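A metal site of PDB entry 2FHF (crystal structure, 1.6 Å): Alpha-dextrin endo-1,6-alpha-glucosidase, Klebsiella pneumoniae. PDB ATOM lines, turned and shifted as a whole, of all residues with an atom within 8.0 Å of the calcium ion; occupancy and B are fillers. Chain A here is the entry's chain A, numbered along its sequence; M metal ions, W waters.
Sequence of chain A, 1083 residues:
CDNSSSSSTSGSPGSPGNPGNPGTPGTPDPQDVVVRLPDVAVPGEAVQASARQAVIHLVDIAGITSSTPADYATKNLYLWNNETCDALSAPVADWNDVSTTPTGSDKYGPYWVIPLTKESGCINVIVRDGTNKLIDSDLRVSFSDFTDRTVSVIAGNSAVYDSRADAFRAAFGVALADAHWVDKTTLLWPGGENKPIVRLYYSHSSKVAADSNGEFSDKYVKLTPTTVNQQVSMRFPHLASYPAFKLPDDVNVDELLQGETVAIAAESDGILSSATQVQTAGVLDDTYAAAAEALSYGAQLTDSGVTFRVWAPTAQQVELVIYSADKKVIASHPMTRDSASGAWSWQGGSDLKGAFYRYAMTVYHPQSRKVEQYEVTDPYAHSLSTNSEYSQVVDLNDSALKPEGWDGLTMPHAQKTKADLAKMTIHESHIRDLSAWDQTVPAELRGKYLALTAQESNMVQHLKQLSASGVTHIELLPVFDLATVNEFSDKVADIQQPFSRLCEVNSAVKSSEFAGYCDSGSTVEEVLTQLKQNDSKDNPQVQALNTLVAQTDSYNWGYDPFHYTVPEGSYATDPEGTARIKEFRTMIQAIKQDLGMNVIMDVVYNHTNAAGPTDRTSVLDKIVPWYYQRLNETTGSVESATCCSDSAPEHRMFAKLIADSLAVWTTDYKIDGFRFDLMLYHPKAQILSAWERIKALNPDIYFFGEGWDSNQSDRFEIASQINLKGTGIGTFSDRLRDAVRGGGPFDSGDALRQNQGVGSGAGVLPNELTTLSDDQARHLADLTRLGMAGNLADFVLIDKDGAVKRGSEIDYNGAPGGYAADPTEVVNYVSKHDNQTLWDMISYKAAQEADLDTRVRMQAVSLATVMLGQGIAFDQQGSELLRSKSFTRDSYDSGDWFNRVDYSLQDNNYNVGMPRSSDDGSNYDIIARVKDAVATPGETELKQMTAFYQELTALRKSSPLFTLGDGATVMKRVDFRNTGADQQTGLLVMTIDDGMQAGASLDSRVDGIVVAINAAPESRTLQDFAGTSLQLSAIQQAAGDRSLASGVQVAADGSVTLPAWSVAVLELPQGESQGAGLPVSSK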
ATOM      1  N   THR A 484      20.668   8.822  20.977  1.00  0.00           N
ATOM      2  CA  THR A 484      20.505  10.269  21.116  1.00  0.00           C
ATOM      3  C   THR A 484      19.293  10.996  20.530  1.00  0.00           C
ATOM      4  O   THR A 484      19.313  12.219  20.379  1.00  0.00           O
ATOM      5  CB  THR A 484      21.794  10.953  20.654  1.00  0.00           C
ATOM      6  OG1 THR A 484      22.200  10.393  19.403  1.00  0.00           O
ATOM      7  CG2 THR A 484      22.896  10.723  21.685  1.00  0.00           C
ATOM      8  N   VAL A 485      18.248  10.245  20.195  1.00  0.00           N
ATOM      9  CA  VAL A 485      17.000  10.817  19.708  1.00  0.00           C
ATOM     10  C   VAL A 485      15.891  10.069  20.435  1.00  0.00           C
ATOM     11  O   VAL A 485      15.860   8.834  20.435  1.00  0.00           O
ATOM     12  CB  VAL A 485      16.823  10.639  18.181  1.00  0.00           C
ATOM     13  CG1 VAL A 485      15.398  10.973  17.775  1.00  0.00           C
ATOM     14  CG2 VAL A 485      17.794  11.559  17.442  1.00  0.00           C
ATOM     15  N   ASN A 486      14.995  10.797  21.088  1.00  0.00           N
ATOM     16  CA  ASN A 486      13.907  10.140  21.799  1.00  0.00           C
ATOM     17  C   ASN A 486      12.902   9.649  20.759  1.00  0.00           C
ATOM     18  O   ASN A 486      12.395  10.432  19.957  1.00  0.00           O
ATOM     19  CB  ASN A 486      13.234  11.101  22.784  1.00  0.00           C
ATOM     20  CG  ASN A 486      12.393  10.381  23.809  1.00  0.00           C
ATOM     21  OD1 ASN A 486      11.671   9.444  23.472  1.00  0.00           O
ATOM     22  ND2 ASN A 486      12.473  10.805  25.062  1.00  0.00           N
ATOM     23  N   ASP A 494      10.291  19.624  16.838  1.00  0.00           N
ATOM     24  CA  ASP A 494      11.146  19.989  15.721  1.00  0.00           C
ATOM     25  C   ASP A 494      10.871  21.419  15.266  1.00  0.00           C
ATOM     26  O   ASP A 494       9.840  21.995  15.597  1.00  0.00           O
ATOM     27  CB  ASP A 494      10.994  18.968  14.583  1.00  0.00           C
ATOM     28  CG  ASP A 494      11.745  17.671  14.876  1.00  0.00           C
ATOM     29  OD1 ASP A 494      12.999  17.732  14.983  1.00  0.00           O
ATOM     30  OD2 ASP A 494      11.106  16.604  15.004  1.00  0.00           O
ATOM     31  N   ASN A 546      19.119  27.543  18.763  1.00  0.00           N
ATOM     32  CA  ASN A 546      19.250  26.212  18.185  1.00  0.00           C
ATOM     33  C   ASN A 546      19.942  25.225  19.115  1.00  0.00           C
ATOM     34  O   ASN A 546      19.668  24.022  19.054  1.00  0.00           O
ATOM     35  CB  ASN A 546      20.005  26.268  16.850  1.00  0.00           C
ATOM     36  CG  ASN A 546      19.714  25.061  15.980  1.00  0.00           C
ATOM     37  OD1 ASN A 546      18.560  24.779  15.671  1.00  0.00           O
ATOM     38  ND2 ASN A 546      20.760  24.335  15.589  1.00  0.00           N
ATOM     39  N   THR A 547      20.838  25.720  19.965  1.00  0.00           N
ATOM     40  CA  THR A 547      21.545  24.839  20.897  1.00  0.00           C
ATOM     41  C   THR A 547      20.562  24.217  21.876  1.00  0.00           C
ATOM     42  O   THR A 547      20.739  23.081  22.309  1.00  0.00           O
ATOM     43  CB  THR A 547      22.637  25.616  21.664  1.00  0.00           C
ATOM     44  OG1 THR A 547      23.667  26.005  20.740  1.00  0.00           O
ATOM     45  CG2 THR A 547      23.259  24.738  22.742  1.00  0.00           C
ATOM     46  N   LEU A 548      19.523  24.965  22.228  1.00  0.00           N
ATOM     47  CA  LEU A 548      18.507  24.459  23.155  1.00  0.00           C
ATOM     48  C   LEU A 548      17.602  23.489  22.388  1.00  0.00           C
ATOM     49  O   LEU A 548      17.249  22.421  22.902  1.00  0.00           O
ATOM     50  CB  LEU A 548      17.690  25.625  23.724  1.00  0.00           C
ATOM     51  CG  LEU A 548      18.486  26.661  24.533  1.00  0.00           C
ATOM     52  CD1 LEU A 548      17.553  27.767  25.017  1.00  0.00           C
ATOM     53  CD2 LEU A 548      19.176  25.987  25.705  1.00  0.00           C
ATOM     54  N   VAL A 549      17.230  23.872  21.162  1.00  0.00           N
ATOM     55  CA  VAL A 549      16.370  23.036  20.321  1.00  0.00           C
ATOM     56  C   VAL A 549      16.969  21.642  20.116  1.00  0.00           C
ATOM     57  O   VAL A 549      16.260  20.642  20.127  1.00  0.00           O
ATOM     58  CB  VAL A 549      16.178  23.694  18.933  1.00  0.00           C
ATOM     59  CG1 VAL A 549      15.454  22.735  17.999  1.00  0.00           C
ATOM     60  CG2 VAL A 549      15.394  25.004  19.066  1.00  0.00           C
ATOM     61  N   ALA A 550      18.282  21.601  19.933  1.00  0.00           N
ATOM     62  CA  ALA A 550      18.999  20.345  19.696  1.00  0.00           C
ATOM     63  C   ALA A 550      18.794  19.272  20.764  1.00  0.00           C
ATOM     64  O   ALA A 550      18.878  18.071  20.472  1.00  0.00           O
ATOM     65  CB  ALA A 550      20.488  20.636  19.532  1.00  0.00           C
ATOM     66  N   GLN A 551      18.546  19.706  21.998  1.00  0.00           N
ATOM     67  CA  GLN A 551      18.357  18.799  23.120  1.00  0.00           C
ATOM     68  C   GLN A 551      17.126  17.907  22.990  1.00  0.00           C
ATOM     69  O   GLN A 551      17.120  16.775  23.492  1.00  0.00           O
ATOM     70  CB  GLN A 551      18.244  19.581  24.435  1.00  0.00           C
ATOM     71  CG  GLN A 551      19.451  20.439  24.761  1.00  0.00           C
ATOM     72  CD  GLN A 551      19.152  21.451  25.859  1.00  0.00           C
ATOM     73  OE1 GLN A 551      20.051  22.132  26.344  1.00  0.00           O
ATOM     74  NE2 GLN A 551      17.891  21.546  26.257  1.00  0.00           N
ATOM     75  N   THR A 552      16.100  18.399  22.320  1.00  0.00           N
ATOM     76  CA  THR A 552      14.856  17.657  22.192  1.00  0.00           C
ATOM     77  C   THR A 552      14.289  17.505  20.779  1.00  0.00           C
ATOM     78  O   THR A 552      13.087  17.264  20.628  1.00  0.00           O
ATOM     79  CB  THR A 552      13.765  18.275  23.104  1.00  0.00           C
ATOM     80  OG1 THR A 552      13.704  19.684  22.883  1.00  0.00           O
ATOM     81  CG2 THR A 552      14.081  18.025  24.582  1.00  0.00           C
ATOM     82  N   ASP A 553      15.122  17.634  19.754  1.00  0.00           N
ATOM     83  CA  ASP A 553      14.636  17.488  18.390  1.00  0.00           C
ATOM     84  C   ASP A 553      14.859  16.066  17.874  1.00  0.00           C
ATOM     85  O   ASP A 553      15.293  15.191  18.628  1.00  0.00           O
ATOM     86  CB  ASP A 553      15.281  18.518  17.440  1.00  0.00           C
ATOM     87  CG  ASP A 553      16.788  18.367  17.314  1.00  0.00           C
ATOM     88  OD1 ASP A 553      17.354  17.346  17.776  1.00  0.00           O
ATOM     89  OD2 ASP A 553      17.426  19.287  16.741  1.00  0.00           O
ATOM     90  N   SER A 554      14.549  15.828  16.606  1.00  0.00           N
ATOM     91  CA  SER A 554      14.716  14.505  16.007  1.00  0.00           C
ATOM     92  C   SER A 554      16.073  14.343  15.346  1.00  0.00           C
ATOM     93  O   SER A 554      16.320  13.337  14.666  1.00  0.00           O
ATOM     94  CB  SER A 554      13.642  14.277  14.938  1.00  0.00           C
ATOM     95  OG  SER A 554      12.328  14.303  15.470  1.00  0.00           O
ATOM     96  N   TYR A 555      16.969  15.304  15.546  1.00  0.00           N
ATOM     97  CA  TYR A 555      18.251  15.278  14.865  1.00  0.00           C
ATOM     98  C   TYR A 555      19.536  14.892  15.602  1.00  0.00           C
ATOM     99  O   TYR A 555      19.839  15.390  16.690  1.00  0.00           O
ATOM    100  CB  TYR A 555      18.497  16.635  14.199  1.00  0.00           C
ATOM    101  CG  TYR A 555      19.594  16.609  13.150  1.00  0.00           C
ATOM    102  CD1 TYR A 555      20.935  16.502  13.507  1.00  0.00           C
ATOM    103  CD2 TYR A 555      19.274  16.593  11.795  1.00  0.00           C
ATOM    104  CE1 TYR A 555      21.928  16.371  12.538  1.00  0.00           C
ATOM    105  CE2 TYR A 555      20.263  16.474  10.813  1.00  0.00           C
ATOM    106  CZ  TYR A 555      21.579  16.350  11.197  1.00  0.00           C
ATOM    107  OH  TYR A 555      22.539  16.171  10.228  1.00  0.00           O
ATOM    108  N   ASN A 556      20.289  13.996  14.970  1.00  0.00           N
ATOM    109  CA  ASN A 556      21.614  13.583  15.444  1.00  0.00           C
ATOM    110  C   ASN A 556      22.228  12.659  14.410  1.00  0.00           C
ATOM    111  O   ASN A 556      21.530  11.831  13.817  1.00  0.00           O
ATOM    112  CB  ASN A 556      21.560  12.873  16.809  1.00  0.00           C
ATOM    113  CG  ASN A 556      22.917  12.869  17.511  1.00  0.00           C
ATOM    114  OD1 ASN A 556      23.875  12.223  17.070  1.00  0.00           O
ATOM    115  ND2 ASN A 556      23.015  13.616  18.614  1.00  0.00           N
ATOM    116  N   TRP A 557      23.523  12.820  14.166  1.00  0.00           N
ATOM    117  CA  TRP A 557      24.197  11.942  13.216  1.00  0.00           C
ATOM    118  C   TRP A 557      23.988  10.501  13.689  1.00  0.00           C
ATOM    119  O   TRP A 557      23.868   9.583  12.882  1.00  0.00           O
ATOM    120  CB  TRP A 557      25.689  12.213  13.178  1.00  0.00           C
ATOM    121  CG  TRP A 557      26.072  13.400  12.374  1.00  0.00           C
ATOM    122  CD1 TRP A 557      25.290  14.095  11.486  1.00  0.00           C
ATOM    123  CD2 TRP A 557      27.353  14.039  12.356  1.00  0.00           C
ATOM    124  NE1 TRP A 557      26.014  15.119  10.920  1.00  0.00           N
ATOM    125  CE2 TRP A 557      27.276  15.104  11.437  1.00  0.00           C
ATOM    126  CE3 TRP A 557      28.558  13.805  13.033  1.00  0.00           C
ATOM    127  CZ2 TRP A 557      28.366  15.951  11.185  1.00  0.00           C
ATOM    128  CZ3 TRP A 557      29.639  14.638  12.779  1.00  0.00           C
ATOM    129  CH2 TRP A 557      29.533  15.699  11.860  1.00  0.00           C
ATOM    130  N   TYR A 892      27.118  17.427  14.162  1.00  0.00           N
ATOM    131  CA  TYR A 892      26.394  16.239  14.645  1.00  0.00           C
ATOM    132  C   TYR A 892      25.089  16.466  15.394  1.00  0.00           C
ATOM    133  O   TYR A 892      24.184  15.635  15.322  1.00  0.00           O
ATOM    134  CB  TYR A 892      27.311  15.363  15.523  1.00  0.00           C
ATOM    135  CG  TYR A 892      27.467  15.862  16.936  1.00  0.00           C
ATOM    136  CD1 TYR A 892      28.218  16.998  17.225  1.00  0.00           C
ATOM    137  CD2 TYR A 892      26.860  15.185  17.998  1.00  0.00           C
ATOM    138  CE1 TYR A 892      28.356  17.460  18.540  1.00  0.00           C
ATOM    139  CE2 TYR A 892      26.992  15.644  19.320  1.00  0.00           C
ATOM    140  CZ  TYR A 892      27.743  16.785  19.580  1.00  0.00           C
ATOM    141  OH  TYR A 892      27.899  17.226  20.870  1.00  0.00           O
ATOM    142  N   ASP A 893      24.999  17.568  16.128  1.00  0.00           N
ATOM    143  CA  ASP A 893      23.812  17.875  16.916  1.00  0.00           C
ATOM    144  C   ASP A 893      23.342  19.294  16.585  1.00  0.00           C
ATOM    145  O   ASP A 893      22.668  19.941  17.398  1.00  0.00           O
ATOM    146  CB  ASP A 893      24.159  17.780  18.410  1.00  0.00           C
ATOM    147  CG  ASP A 893      22.929  17.617  19.296  1.00  0.00           C
ATOM    148  OD1 ASP A 893      23.087  17.746  20.537  1.00  0.00           O
ATOM    149  OD2 ASP A 893      21.831  17.351  18.781  1.00  0.00           O
ATOM    150  N   SER A 894      23.683  19.762  15.390  1.00  0.00           N
ATOM    151  CA  SER A 894      23.307  21.116  14.975  1.00  0.00           C
ATOM    152  C   SER A 894      21.954  21.229  14.297  1.00  0.00           C
ATOM    153  O   SER A 894      21.603  22.265  13.731  1.00  0.00           O
ATOM    154  CB  SER A 894      24.403  21.718  14.090  1.00  0.00           C
ATOM    155  OG  SER A 894      25.539  22.046  14.871  1.00  0.00           O
ATOM    156  N   GLY A 895      21.194  20.131  14.351  1.00  0.00           N
ATOM    157  CA  GLY A 895      19.841  20.110  13.802  1.00  0.00           C
ATOM    158  C   GLY A 895      19.566  20.301  12.328  1.00  0.00           C
ATOM    159  O   GLY A 895      20.476  20.344  11.488  1.00  0.00           O
ATOM    160  N   ASP A 896      18.283  20.396  12.003  1.00  0.00           N
ATOM    161  CA  ASP A 896      17.845  20.595  10.635  1.00  0.00           C
ATOM    162  C   ASP A 896      18.331  21.942  10.083  1.00  0.00           C
ATOM    163  O   ASP A 896      18.586  22.080   8.895  1.00  0.00           O
ATOM    164  CB  ASP A 896      16.319  20.588  10.529  1.00  0.00           C
ATOM    165  CG  ASP A 896      15.690  19.228  10.775  1.00  0.00           C
ATOM    166  OD1 ASP A 896      16.377  18.190  10.609  1.00  0.00           O
ATOM    167  OD2 ASP A 896      14.493  19.183  11.121  1.00  0.00           O
HETATM  168 CA    CA M   1      19.513  16.654  18.658  1.00  0.00          CA
HETATM  169  O   HOH W   1      19.932  18.607  17.029  1.00  0.00           O
HETATM  170  O   HOH W   2      20.636  14.761  19.857  1.00  0.00           O
HETATM  171  O   HOH W   3      17.897  15.175  19.462  1.00  0.00           O
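The nearest printed residue that does not touch the calcium ion is Asn 556 (4.6 Å).
Water W3 binds the calcium ion (2.3 Å).
The backbone carbonyl oxygen (O) of Tyr 555 is bound to the calcium ion (2.4 Å).
The calcium ion is bound by O of Ala 550.
The calcium ion is bound by the side-chain carboxylate (OD2) of Asp 893.
OD1 of Asp 553 is bound to the calcium ion.
The calcium ion is bound by water W2 (2.5 Å).
Water W1 binds the calcium ion, 2.6 Å away.
Water W2 lies within hydrogen-bond range of the backbone carbonyl oxygen of Thr 484 and the side-chain amide nitrogen of Asn 556.
Water W3 lies within hydrogen-bond range of the backbone carbonyl oxygen of Asp 553 (2.7 Å) and the backbone carbonyl oxygen of Thr 484 (3.4 Å).
Water W1 lies within hydrogen-bond range of OD2 of Asp 553, O of Asp 893 and N of Gly 895.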
